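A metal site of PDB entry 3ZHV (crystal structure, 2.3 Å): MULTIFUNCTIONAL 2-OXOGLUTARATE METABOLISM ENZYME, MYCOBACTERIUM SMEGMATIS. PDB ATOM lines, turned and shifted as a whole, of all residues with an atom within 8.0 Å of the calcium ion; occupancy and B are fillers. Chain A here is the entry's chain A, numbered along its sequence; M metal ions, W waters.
The calcium ion is bound by water W1, the backbone carbonyl oxygen (O) of Ile 701, the backbone carbonyl oxygen (O) of His 696, the side-chain carboxylate (OD2) of Asp 645, the side-chain carboxylate (OD1) of Asp 699, water W2 and the side-chain carboxylate (OD1) of Asp 645.
The calcium ion has seven donor atoms within binding distance.
Water W1 lies within hydrogen-bond range of OD2 of Asp 699 (2.6 Å) and ND1 of His 696 (3.2 Å).
Within 4 Å of the calcium ion: Asp 645, His 696, Asp 699 and Ile 701.
OD1 of Asp 645 sits close to N of Arg 703, at 3.0 Å.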
ATOM      1  N   LYS A 535     -31.317   0.003  -5.595  1.00  0.00           N
ATOM      2  CA  LYS A 535     -30.498  -0.092  -4.388  1.00  0.00           C
ATOM      3  C   LYS A 535     -31.312  -0.372  -3.133  1.00  0.00           C
ATOM      4  O   LYS A 535     -32.403   0.165  -2.960  1.00  0.00           O
ATOM      5  CB  LYS A 535     -29.686   1.199  -4.166  1.00  0.00           C
ATOM      6  CG  LYS A 535     -28.344   0.924  -3.523  1.00  0.00           C
ATOM      7  CD  LYS A 535     -27.480   2.148  -3.458  1.00  0.00           C
ATOM      8  CE  LYS A 535     -26.189   1.874  -2.745  1.00  0.00           C
ATOM      9  NZ  LYS A 535     -25.277   1.007  -3.534  1.00  0.00           N
ATOM     10  N   PRO A 608     -22.178  -4.873   0.937  1.00  0.00           N
ATOM     11  CA  PRO A 608     -21.474  -3.684   0.418  1.00  0.00           C
ATOM     12  C   PRO A 608     -22.279  -2.888  -0.606  1.00  0.00           C
ATOM     13  O   PRO A 608     -21.920  -1.753  -0.901  1.00  0.00           O
ATOM     14  CB  PRO A 608     -20.206  -4.274  -0.228  1.00  0.00           C
ATOM     15  CG  PRO A 608     -20.097  -5.675   0.287  1.00  0.00           C
ATOM     16  CD  PRO A 608     -21.496  -6.120   0.508  1.00  0.00           C
ATOM     17  N   ALA A 610     -25.545  -2.196  -0.275  1.00  0.00           N
ATOM     18  CA  ALA A 610     -26.613  -1.498   0.420  1.00  0.00           C
ATOM     19  C   ALA A 610     -26.184  -0.096   0.801  1.00  0.00           C
ATOM     20  O   ALA A 610     -25.005   0.144   1.068  1.00  0.00           O
ATOM     21  CB  ALA A 610     -27.012  -2.270   1.668  1.00  0.00           C
ATOM     22  N   MET A 611     -27.152   0.836   0.811  1.00  0.00           N
ATOM     23  CA  MET A 611     -26.993   2.218   1.278  1.00  0.00           C
ATOM     24  C   MET A 611     -27.415   2.161   2.742  1.00  0.00           C
ATOM     25  O   MET A 611     -28.582   1.894   3.013  1.00  0.00           O
ATOM     26  CB  MET A 611     -27.840   3.197   0.418  1.00  0.00           C
ATOM     27  CG  MET A 611     -27.774   4.653   0.859  1.00  0.00           C
ATOM     28  SD  MET A 611     -26.342   5.564   0.213  1.00  0.00           S
ATOM     29  CE  MET A 611     -26.722   7.180   0.804  1.00  0.00           C
ATOM     30  N   SER A 644     -16.187  -0.484   4.641  1.00  0.00           N
ATOM     31  CA  SER A 644     -17.536  -0.076   5.028  1.00  0.00           C
ATOM     32  C   SER A 644     -17.937   1.192   4.318  1.00  0.00           C
ATOM     33  O   SER A 644     -17.142   2.124   4.250  1.00  0.00           O
ATOM     34  CB  SER A 644     -17.626   0.146   6.536  1.00  0.00           C
ATOM     35  OG  SER A 644     -18.952   0.434   6.916  1.00  0.00           O
ATOM     36  N   ASP A 645     -19.174   1.236   3.802  1.00  0.00           N
ATOM     37  CA  ASP A 645     -19.787   2.401   3.164  1.00  0.00           C
ATOM     38  C   ASP A 645     -20.849   2.980   4.104  1.00  0.00           C
ATOM     39  O   ASP A 645     -21.798   3.604   3.642  1.00  0.00           O
ATOM     40  CB  ASP A 645     -20.394   2.027   1.795  1.00  0.00           C
ATOM     41  CG  ASP A 645     -20.280   3.118   0.734  1.00  0.00           C
ATOM     42  OD1 ASP A 645     -19.229   3.817   0.698  1.00  0.00           O
ATOM     43  OD2 ASP A 645     -21.189   3.209  -0.117  1.00  0.00           O
ATOM     44  N   VAL A 646     -20.702   2.764   5.414  1.00  0.00           N
ATOM     45  CA  VAL A 646     -21.679   3.265   6.398  1.00  0.00           C
ATOM     46  C   VAL A 646     -21.727   4.793   6.410  1.00  0.00           C
ATOM     47  O   VAL A 646     -20.693   5.446   6.263  1.00  0.00           O
ATOM     48  CB  VAL A 646     -21.457   2.694   7.840  1.00  0.00           C
ATOM     49  CG1 VAL A 646     -20.176   3.217   8.508  1.00  0.00           C
ATOM     50  CG2 VAL A 646     -22.685   2.912   8.734  1.00  0.00           C
ATOM     51  N   VAL A 647     -22.939   5.352   6.540  1.00  0.00           N
ATOM     52  CA  VAL A 647     -23.173   6.787   6.649  1.00  0.00           C
ATOM     53  C   VAL A 647     -23.601   7.107   8.061  1.00  0.00           C
ATOM     54  O   VAL A 647     -24.534   6.472   8.570  1.00  0.00           O
ATOM     55  CB  VAL A 647     -24.246   7.308   5.630  1.00  0.00           C
ATOM     56  CG1 VAL A 647     -24.398   8.823   5.697  1.00  0.00           C
ATOM     57  CG2 VAL A 647     -23.960   6.849   4.196  1.00  0.00           C
ATOM     58  N   THR A 679     -15.087  10.143   4.290  1.00  0.00           N
ATOM     59  CA  THR A 679     -15.521  11.386   3.659  1.00  0.00           C
ATOM     60  C   THR A 679     -16.253  12.148   4.759  1.00  0.00           C
ATOM     61  O   THR A 679     -17.093  11.554   5.454  1.00  0.00           O
ATOM     62  CB  THR A 679     -16.353  11.160   2.369  1.00  0.00           C
ATOM     63  OG1 THR A 679     -15.646  10.287   1.460  1.00  0.00           O
ATOM     64  CG2 THR A 679     -16.690  12.472   1.654  1.00  0.00           C
ATOM     65  N   LEU A 692     -24.585  14.535  -2.576  1.00  0.00           N
ATOM     66  CA  LEU A 692     -23.617  13.897  -1.682  1.00  0.00           C
ATOM     67  C   LEU A 692     -24.036  12.430  -1.404  1.00  0.00           C
ATOM     68  O   LEU A 692     -23.194  11.528  -1.467  1.00  0.00           O
ATOM     69  CB  LEU A 692     -23.519  14.694  -0.343  1.00  0.00           C
ATOM     70  CG  LEU A 692     -22.569  14.130   0.735  1.00  0.00           C
ATOM     71  CD1 LEU A 692     -21.114  14.485   0.442  1.00  0.00           C
ATOM     72  CD2 LEU A 692     -22.985  14.589   2.105  1.00  0.00           C
ATOM     73  N   LEU A 693     -25.342  12.187  -1.093  1.00  0.00           N
ATOM     74  CA  LEU A 693     -25.882  10.854  -0.812  1.00  0.00           C
ATOM     75  C   LEU A 693     -25.882   9.992  -2.074  1.00  0.00           C
ATOM     76  O   LEU A 693     -25.499   8.816  -2.018  1.00  0.00           O
ATOM     77  CB  LEU A 693     -27.304  10.922  -0.225  1.00  0.00           C
ATOM     78  CG  LEU A 693     -27.481  11.544   1.171  1.00  0.00           C
ATOM     79  CD1 LEU A 693     -28.971  11.518   1.577  1.00  0.00           C
ATOM     80  CD2 LEU A 693     -26.627  10.823   2.239  1.00  0.00           C
ATOM     81  N   ARG A 694     -26.271  10.568  -3.223  1.00  0.00           N
ATOM     82  CA  ARG A 694     -26.282   9.840  -4.493  1.00  0.00           C
ATOM     83  C   ARG A 694     -24.859   9.479  -4.924  1.00  0.00           C
ATOM     84  O   ARG A 694     -24.639   8.326  -5.321  1.00  0.00           O
ATOM     85  CB  ARG A 694     -27.041  10.611  -5.585  1.00  0.00           C
ATOM     86  CG  ARG A 694     -28.541  10.461  -5.380  1.00  0.00           C
ATOM     87  CD  ARG A 694     -29.407  10.992  -6.502  1.00  0.00           C
ATOM     88  NE  ARG A 694     -29.061  10.473  -7.830  1.00  0.00           N
ATOM     89  CZ  ARG A 694     -29.373   9.260  -8.262  1.00  0.00           C
ATOM     90  NH1 ARG A 694     -30.020   8.411  -7.477  1.00  0.00           N
ATOM     91  NH2 ARG A 694     -29.030   8.887  -9.489  1.00  0.00           N
ATOM     92  N   ARG A 695     -23.875  10.403  -4.781  1.00  0.00           N
ATOM     93  CA  ARG A 695     -22.477  10.108  -5.123  1.00  0.00           C
ATOM     94  C   ARG A 695     -21.974   8.964  -4.253  1.00  0.00           C
ATOM     95  O   ARG A 695     -21.400   8.014  -4.768  1.00  0.00           O
ATOM     96  CB  ARG A 695     -21.582  11.371  -4.977  1.00  0.00           C
ATOM     97  CG  ARG A 695     -20.084  11.110  -5.244  1.00  0.00           C
ATOM     98  CD  ARG A 695     -19.220  12.343  -4.986  1.00  0.00           C
ATOM     99  NE  ARG A 695     -19.099  12.647  -3.557  1.00  0.00           N
ATOM    100  CZ  ARG A 695     -18.189  13.452  -3.020  1.00  0.00           C
ATOM    101  NH1 ARG A 695     -17.304  14.074  -3.790  1.00  0.00           N
ATOM    102  NH2 ARG A 695     -18.157  13.667  -1.712  1.00  0.00           N
ATOM    103  N   HIS A 696     -22.269   9.019  -2.938  1.00  0.00           N
ATOM    104  CA  HIS A 696     -21.862   8.006  -1.965  1.00  0.00           C
ATOM    105  C   HIS A 696     -22.432   6.620  -2.309  1.00  0.00           C
ATOM    106  O   HIS A 696     -21.715   5.637  -2.190  1.00  0.00           O
ATOM    107  CB  HIS A 696     -22.287   8.409  -0.548  1.00  0.00           C
ATOM    108  CG  HIS A 696     -21.841   7.442   0.489  1.00  0.00           C
ATOM    109  ND1 HIS A 696     -20.514   7.344   0.878  1.00  0.00           N
ATOM    110  CD2 HIS A 696     -22.549   6.485   1.136  1.00  0.00           C
ATOM    111  CE1 HIS A 696     -20.483   6.380   1.792  1.00  0.00           C
ATOM    112  NE2 HIS A 696     -21.682   5.835   1.962  1.00  0.00           N
ATOM    113  N   GLY A 697     -23.680   6.562  -2.738  1.00  0.00           N
ATOM    114  CA  GLY A 697     -24.323   5.304  -3.094  1.00  0.00           C
ATOM    115  C   GLY A 697     -23.949   4.745  -4.445  1.00  0.00           C
ATOM    116  O   GLY A 697     -24.088   3.541  -4.657  1.00  0.00           O
ATOM    117  N   LYS A 698     -23.467   5.595  -5.353  1.00  0.00           N
ATOM    118  CA  LYS A 698     -23.182   5.176  -6.720  1.00  0.00           C
ATOM    119  C   LYS A 698     -21.684   5.175  -7.130  1.00  0.00           C
ATOM    120  O   LYS A 698     -21.384   4.736  -8.238  1.00  0.00           O
ATOM    121  CB  LYS A 698     -23.940   6.101  -7.706  1.00  0.00           C
ATOM    122  CG  LYS A 698     -25.467   6.018  -7.627  1.00  0.00           C
ATOM    123  CD  LYS A 698     -26.144   7.129  -8.455  1.00  0.00           C
ATOM    124  CE  LYS A 698     -26.151   6.889  -9.952  1.00  0.00           C
ATOM    125  NZ  LYS A 698     -26.939   5.685 -10.317  1.00  0.00           N
ATOM    126  N   ASP A 699     -20.757   5.659  -6.260  1.00  0.00           N
ATOM    127  CA  ASP A 699     -19.336   5.809  -6.599  1.00  0.00           C
ATOM    128  C   ASP A 699     -18.515   4.482  -6.680  1.00  0.00           C
ATOM    129  O   ASP A 699     -17.321   4.535  -7.018  1.00  0.00           O
ATOM    130  CB  ASP A 699     -18.644   6.785  -5.613  1.00  0.00           C
ATOM    131  CG  ASP A 699     -18.670   6.402  -4.146  1.00  0.00           C
ATOM    132  OD1 ASP A 699     -19.045   5.245  -3.842  1.00  0.00           O
ATOM    133  OD2 ASP A 699     -18.267   7.245  -3.309  1.00  0.00           O
ATOM    134  N   GLY A 700     -19.134   3.352  -6.333  1.00  0.00           N
ATOM    135  CA  GLY A 700     -18.489   2.032  -6.351  1.00  0.00           C
ATOM    136  C   GLY A 700     -17.301   1.880  -5.416  1.00  0.00           C
ATOM    137  O   GLY A 700     -16.484   0.976  -5.592  1.00  0.00           O
ATOM    138  N   ILE A 701     -17.207   2.782  -4.417  1.00  0.00           N
ATOM    139  CA  ILE A 701     -16.140   2.882  -3.419  1.00  0.00           C
ATOM    140  C   ILE A 701     -16.745   2.674  -2.033  1.00  0.00           C
ATOM    141  O   ILE A 701     -17.790   3.254  -1.727  1.00  0.00           O
ATOM    142  CB  ILE A 701     -15.421   4.269  -3.599  1.00  0.00           C
ATOM    143  CG1 ILE A 701     -14.273   4.131  -4.613  1.00  0.00           C
ATOM    144  CG2 ILE A 701     -14.935   4.892  -2.281  1.00  0.00           C
ATOM    145  CD1 ILE A 701     -13.918   5.453  -5.402  1.00  0.00           C
ATOM    146  N   GLN A 702     -16.090   1.841  -1.194  1.00  0.00           N
ATOM    147  CA  GLN A 702     -16.578   1.553   0.136  1.00  0.00           C
ATOM    148  C   GLN A 702     -15.804   2.400   1.148  1.00  0.00           C
ATOM    149  O   GLN A 702     -14.713   2.024   1.612  1.00  0.00           O
ATOM    150  CB  GLN A 702     -16.525   0.044   0.436  1.00  0.00           C
ATOM    151  CG  GLN A 702     -17.158  -0.850  -0.646  1.00  0.00           C
ATOM    152  CD  GLN A 702     -18.647  -0.677  -0.785  1.00  0.00           C
ATOM    153  OE1 GLN A 702     -19.398  -0.947   0.151  1.00  0.00           O
ATOM    154  NE2 GLN A 702     -19.108  -0.242  -1.951  1.00  0.00           N
ATOM    155  N   ARG A 703     -16.366   3.570   1.467  1.00  0.00           N
ATOM    156  CA  ARG A 703     -15.764   4.502   2.413  1.00  0.00           C
ATOM    157  C   ARG A 703     -16.837   5.113   3.326  1.00  0.00           C
ATOM    158  O   ARG A 703     -17.854   5.622   2.844  1.00  0.00           O
ATOM    159  CB  ARG A 703     -15.021   5.602   1.623  1.00  0.00           C
ATOM    160  CG  ARG A 703     -14.069   6.492   2.429  1.00  0.00           C
ATOM    161  CD  ARG A 703     -13.111   7.234   1.502  1.00  0.00           C
ATOM    162  NE  ARG A 703     -12.209   6.291   0.820  1.00  0.00           N
ATOM    163  CZ  ARG A 703     -11.515   6.566  -0.283  1.00  0.00           C
ATOM    164  NH1 ARG A 703     -11.586   7.763  -0.847  1.00  0.00           N
ATOM    165  NH2 ARG A 703     -10.747   5.631  -0.826  1.00  0.00           N
ATOM    166  N   PRO A 704     -16.620   5.129   4.646  1.00  0.00           N
ATOM    167  CA  PRO A 704     -17.622   5.763   5.517  1.00  0.00           C
ATOM    168  C   PRO A 704     -17.793   7.234   5.213  1.00  0.00           C
ATOM    169  O   PRO A 704     -16.843   7.903   4.834  1.00  0.00           O
ATOM    170  CB  PRO A 704     -17.069   5.539   6.922  1.00  0.00           C
ATOM    171  CG  PRO A 704     -16.139   4.322   6.762  1.00  0.00           C
ATOM    172  CD  PRO A 704     -15.507   4.557   5.440  1.00  0.00           C
ATOM    173  N   LEU A 705     -19.042   7.716   5.291  1.00  0.00           N
ATOM    174  CA  LEU A 705     -19.416   9.099   5.068  1.00  0.00           C
ATOM    175  C   LEU A 705     -19.943   9.669   6.382  1.00  0.00           C
ATOM    176  O   LEU A 705     -20.858   9.093   6.974  1.00  0.00           O
ATOM    177  CB  LEU A 705     -20.449   9.218   3.927  1.00  0.00           C
ATOM    178  CG  LEU A 705     -21.103  10.606   3.681  1.00  0.00           C
ATOM    179  CD1 LEU A 705     -20.088  11.644   3.174  1.00  0.00           C
ATOM    180  CD2 LEU A 705     -22.247  10.508   2.708  1.00  0.00           C
HETATM  181 CA    CA M   1     -19.798   4.351  -1.686  1.00  0.00          CA
HETATM  182  O   HOH W   1     -18.373   5.863  -1.064  1.00  0.00           O
HETATM  183  O   HOH W   2     -20.979   2.577  -2.921  1.00  0.00           O
